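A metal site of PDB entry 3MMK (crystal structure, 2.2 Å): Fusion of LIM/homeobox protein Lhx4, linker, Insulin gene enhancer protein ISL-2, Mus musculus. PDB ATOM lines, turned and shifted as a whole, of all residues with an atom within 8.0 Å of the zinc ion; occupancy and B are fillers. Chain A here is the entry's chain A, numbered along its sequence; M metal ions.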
ATOM      1  N   GLN A   8       1.620  17.103 -18.951  1.00  0.00           N
ATOM      2  CA  GLN A   8       0.842  15.940 -19.334  1.00  0.00           C
ATOM      3  C   GLN A   8       1.363  14.737 -18.569  1.00  0.00           C
ATOM      4  O   GLN A   8       2.572  14.555 -18.433  1.00  0.00           O
ATOM      5  CB  GLN A   8       0.911  15.693 -20.835  1.00  0.00           C
ATOM      6  CG  GLN A   8       0.443  16.883 -21.649  1.00  0.00           C
ATOM      7  CD  GLN A   8       0.637  16.683 -23.129  1.00  0.00           C
ATOM      8  OE1 GLN A   8       1.241  17.501 -23.804  1.00  0.00           O
ATOM      9  NE2 GLN A   8       0.110  15.576 -23.654  1.00  0.00           N
ATOM     10  N   CYS A   9       0.448  13.923 -18.072  1.00  0.00           N
ATOM     11  CA  CYS A   9       0.795  12.780 -17.243  1.00  0.00           C
ATOM     12  C   CYS A   9       1.700  11.801 -17.991  1.00  0.00           C
ATOM     13  O   CYS A   9       1.420  11.413 -19.123  1.00  0.00           O
ATOM     14  CB  CYS A   9      -0.480  12.088 -16.764  1.00  0.00           C
ATOM     15  SG  CYS A   9      -0.211  10.776 -15.585  1.00  0.00           S
ATOM     16  N   ALA A  10       2.797  11.391 -17.359  1.00  0.00           N
ATOM     17  CA  ALA A  10       3.712  10.416 -17.947  1.00  0.00           C
ATOM     18  C   ALA A  10       2.986   9.099 -18.198  1.00  0.00           C
ATOM     19  O   ALA A  10       3.327   8.354 -19.123  1.00  0.00           O
ATOM     20  CB  ALA A  10       4.922  10.195 -17.042  1.00  0.00           C
ATOM     21  N   GLY A  11       1.985   8.818 -17.372  1.00  0.00           N
ATOM     22  CA  GLY A  11       1.207   7.595 -17.495  1.00  0.00           C
ATOM     23  C   GLY A  11       0.144   7.642 -18.579  1.00  0.00           C
ATOM     24  O   GLY A  11       0.190   6.846 -19.523  1.00  0.00           O
ATOM     25  N   CYS A  12      -0.798   8.576 -18.460  1.00  0.00           N
ATOM     26  CA  CYS A  12      -1.952   8.628 -19.361  1.00  0.00           C
ATOM     27  C   CYS A  12      -1.821   9.678 -20.461  1.00  0.00           C
ATOM     28  O   CYS A  12      -2.665   9.773 -21.352  1.00  0.00           O
ATOM     29  CB  CYS A  12      -3.224   8.886 -18.557  1.00  0.00           C
ATOM     30  SG  CYS A  12      -3.383  10.595 -17.989  1.00  0.00           S
ATOM     31  N   ASN A  13      -0.764  10.477 -20.380  1.00  0.00           N
ATOM     32  CA  ASN A  13      -0.477  11.535 -21.358  1.00  0.00           C
ATOM     33  C   ASN A  13      -1.523  12.649 -21.416  1.00  0.00           C
ATOM     34  O   ASN A  13      -1.445  13.540 -22.277  1.00  0.00           O
ATOM     35  CB  ASN A  13      -0.260  10.938 -22.758  1.00  0.00           C
ATOM     36  CG  ASN A  13       0.522  11.877 -23.665  1.00  0.00           C
ATOM     37  OD1 ASN A  13       1.384  12.617 -23.202  1.00  0.00           O
ATOM     38  ND2 ASN A  13       0.214  11.841 -24.952  1.00  0.00           N
ATOM     39  N   GLN A  14      -2.479  12.623 -20.503  1.00  0.00           N
ATOM     40  CA  GLN A  14      -3.483  13.678 -20.422  1.00  0.00           C
ATOM     41  C   GLN A  14      -2.967  14.833 -19.580  1.00  0.00           C
ATOM     42  O   GLN A  14      -2.076  14.663 -18.755  1.00  0.00           O
ATOM     43  CB  GLN A  14      -4.800  13.156 -19.842  1.00  0.00           C
ATOM     44  CG  GLN A  14      -5.452  12.056 -20.660  1.00  0.00           C
ATOM     45  CD  GLN A  14      -6.749  11.564 -20.053  1.00  0.00           C
ATOM     46  OE1 GLN A  14      -7.303  12.202 -19.154  1.00  0.00           O
ATOM     47  NE2 GLN A  14      -7.249  10.443 -20.543  1.00  0.00           N
ATOM     48  N   HIS A  15      -3.531  16.020 -19.793  1.00  0.00           N
ATOM     49  CA  HIS A  15      -3.156  17.185 -19.001  1.00  0.00           C
ATOM     50  C   HIS A  15      -3.622  17.021 -17.547  1.00  0.00           C
ATOM     51  O   HIS A  15      -4.757  16.626 -17.283  1.00  0.00           O
ATOM     52  CB  HIS A  15      -3.721  18.470 -19.614  1.00  0.00           C
ATOM     53  CG  HIS A  15      -2.983  18.926 -20.829  1.00  0.00           C
ATOM     54  ND1 HIS A  15      -3.473  18.748 -22.105  1.00  0.00           N
ATOM     55  CD2 HIS A  15      -1.780  19.530 -20.973  1.00  0.00           C
ATOM     56  CE1 HIS A  15      -2.609  19.234 -22.974  1.00  0.00           C
ATOM     57  NE2 HIS A  15      -1.569  19.716 -22.317  1.00  0.00           N
ATOM     58  N   ILE A  16      -2.723  17.335 -16.620  1.00  0.00           N
ATOM     59  CA  ILE A  16      -2.995  17.142 -15.202  1.00  0.00           C
ATOM     60  C   ILE A  16      -3.577  18.400 -14.585  1.00  0.00           C
ATOM     61  O   ILE A  16      -2.870  19.404 -14.412  1.00  0.00           O
ATOM     62  CB  ILE A  16      -1.729  16.714 -14.448  1.00  0.00           C
ATOM     63  CG1 ILE A  16      -1.171  15.404 -15.019  1.00  0.00           C
ATOM     64  CG2 ILE A  16      -2.018  16.555 -12.962  1.00  0.00           C
ATOM     65  CD1 ILE A  16       0.156  14.971 -14.413  1.00  0.00           C
ATOM     66  N   ASP A  18      -5.142  18.315 -11.598  1.00  0.00           N
ATOM     67  CA  ASP A  18      -5.114  18.120 -10.150  1.00  0.00           C
ATOM     68  C   ASP A  18      -4.265  19.207  -9.504  1.00  0.00           C
ATOM     69  O   ASP A  18      -3.216  19.571 -10.028  1.00  0.00           O
ATOM     70  CB  ASP A  18      -4.518  16.755  -9.796  1.00  0.00           C
ATOM     71  CG  ASP A  18      -5.441  15.597 -10.147  1.00  0.00           C
ATOM     72  OD1 ASP A  18      -4.978  14.438 -10.123  1.00  0.00           O
ATOM     73  OD2 ASP A  18      -6.630  15.850 -10.460  1.00  0.00           O
ATOM     74  N   HIS A  28       6.013  13.923 -14.771  1.00  0.00           N
ATOM     75  CA  HIS A  28       4.842  14.280 -13.970  1.00  0.00           C
ATOM     76  C   HIS A  28       3.709  13.263 -14.073  1.00  0.00           C
ATOM     77  O   HIS A  28       3.527  12.627 -15.107  1.00  0.00           O
ATOM     78  CB  HIS A  28       4.361  15.681 -14.357  1.00  0.00           C
ATOM     79  CG  HIS A  28       5.379  16.749 -14.129  1.00  0.00           C
ATOM     80  ND1 HIS A  28       6.252  17.167 -15.114  1.00  0.00           N
ATOM     81  CD2 HIS A  28       5.677  17.478 -13.029  1.00  0.00           C
ATOM     82  CE1 HIS A  28       7.030  18.116 -14.632  1.00  0.00           C
ATOM     83  NE2 HIS A  28       6.702  18.324 -13.375  1.00  0.00           N
ATOM     84  N   TRP A  29       2.955  13.123 -12.985  1.00  0.00           N
ATOM     85  CA  TRP A  29       1.938  12.077 -12.873  1.00  0.00           C
ATOM     86  C   TRP A  29       0.679  12.548 -12.164  1.00  0.00           C
ATOM     87  O   TRP A  29       0.743  13.338 -11.225  1.00  0.00           O
ATOM     88  CB  TRP A  29       2.483  10.898 -12.069  1.00  0.00           C
ATOM     89  CG  TRP A  29       3.478  10.050 -12.780  1.00  0.00           C
ATOM     90  CD1 TRP A  29       4.809  10.292 -12.931  1.00  0.00           C
ATOM     91  CD2 TRP A  29       3.212   8.792 -13.422  1.00  0.00           C
ATOM     92  NE1 TRP A  29       5.394   9.272 -13.643  1.00  0.00           N
ATOM     93  CE2 TRP A  29       4.433   8.334 -13.950  1.00  0.00           C
ATOM     94  CE3 TRP A  29       2.065   8.022 -13.609  1.00  0.00           C
ATOM     95  CZ2 TRP A  29       4.538   7.142 -14.648  1.00  0.00           C
ATOM     96  CZ3 TRP A  29       2.168   6.835 -14.295  1.00  0.00           C
ATOM     97  CH2 TRP A  29       3.398   6.404 -14.811  1.00  0.00           C
ATOM     98  N   HIS A  30      -0.464  12.031 -12.606  1.00  0.00           N
ATOM     99  CA  HIS A  30      -1.661  12.051 -11.767  1.00  0.00           C
ATOM    100  C   HIS A  30      -1.379  11.139 -10.594  1.00  0.00           C
ATOM    101  O   HIS A  30      -0.684  10.129 -10.736  1.00  0.00           O
ATOM    102  CB  HIS A  30      -2.868  11.501 -12.536  1.00  0.00           C
ATOM    103  CG  HIS A  30      -3.518  12.485 -13.450  1.00  0.00           C
ATOM    104  ND1 HIS A  30      -3.467  12.371 -14.820  1.00  0.00           N
ATOM    105  CD2 HIS A  30      -4.247  13.590 -13.193  1.00  0.00           C
ATOM    106  CE1 HIS A  30      -4.129  13.369 -15.369  1.00  0.00           C
ATOM    107  NE2 HIS A  30      -4.615  14.134 -14.404  1.00  0.00           N
ATOM    108  N   SER A  31      -1.910  11.479  -9.424  1.00  0.00           N
ATOM    109  CA  SER A  31      -1.818  10.593  -8.269  1.00  0.00           C
ATOM    110  C   SER A  31      -2.446   9.254  -8.614  1.00  0.00           C
ATOM    111  O   SER A  31      -1.926   8.203  -8.252  1.00  0.00           O
ATOM    112  CB  SER A  31      -2.552  11.197  -7.070  1.00  0.00           C
ATOM    113  OG  SER A  31      -1.974  12.427  -6.670  1.00  0.00           O
ATOM    114  N   SER A  32      -3.571   9.300  -9.316  1.00  0.00           N
ATOM    115  CA  SER A  32      -4.356   8.107  -9.622  1.00  0.00           C
ATOM    116  C   SER A  32      -3.759   7.293 -10.760  1.00  0.00           C
ATOM    117  O   SER A  32      -4.266   6.214 -11.089  1.00  0.00           O
ATOM    118  CB  SER A  32      -5.796   8.492  -9.974  1.00  0.00           C
ATOM    119  OG  SER A  32      -5.863   9.087 -11.260  1.00  0.00           O
ATOM    120  N   CYS A  33      -2.691   7.800 -11.378  1.00  0.00           N
ATOM    121  CA  CYS A  33      -2.001   7.060 -12.428  1.00  0.00           C
ATOM    122  C   CYS A  33      -0.706   6.426 -11.934  1.00  0.00           C
ATOM    123  O   CYS A  33      -0.141   5.557 -12.596  1.00  0.00           O
ATOM    124  CB  CYS A  33      -1.757   7.950 -13.647  1.00  0.00           C
ATOM    125  SG  CYS A  33      -3.252   8.341 -14.576  1.00  0.00           S
ATOM    126  N   LEU A  34      -0.227   6.869 -10.775  1.00  0.00           N
ATOM    127  CA  LEU A  34       0.940   6.272 -10.143  1.00  0.00           C
ATOM    128  C   LEU A  34       0.554   5.091  -9.263  1.00  0.00           C
ATOM    129  O   LEU A  34       0.570   5.189  -8.042  1.00  0.00           O
ATOM    130  CB  LEU A  34       1.710   7.308  -9.307  1.00  0.00           C
ATOM    131  CG  LEU A  34       3.000   7.858  -9.913  1.00  0.00           C
ATOM    132  CD1 LEU A  34       3.701   8.762  -8.910  1.00  0.00           C
ATOM    133  CD2 LEU A  34       3.916   6.735 -10.332  1.00  0.00           C
HETATM  134 ZN    ZN M   1      -2.562  10.310 -15.715  1.00  0.00          ZN
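The side-chain sulfur (SG) of Cys 9 lies close to the backbone NH (N) of Gly 11 (3.4 Å). O of Gln 14 sits at hydrogen-bond distance from N of Cys 9, at 2.7 Å. The backbone NH (N) of Gln 14 sits close to the side-chain sulfur (SG) of Cys 12.
SG of Cys 33 is bound to the zinc ion (2.4 Å). The side-chain sulfur (SG) of Cys 9 is bound to the zinc ion. ND1 of His 30 binds the zinc ion (2.4 Å). The zinc ion is bound by the side-chain sulfur (SG) of Cys 12 (2.4 Å).
Four residues have an atom within 4 Å of the zinc ion: Cys 9, Cys 12, His 30 and Cys 33. Along chain A the residues within 4 Å of the zinc ion span positions 9 to 33. The nearest printed residue that does not touch the zinc ion is Gly 11 (4.8 Å).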
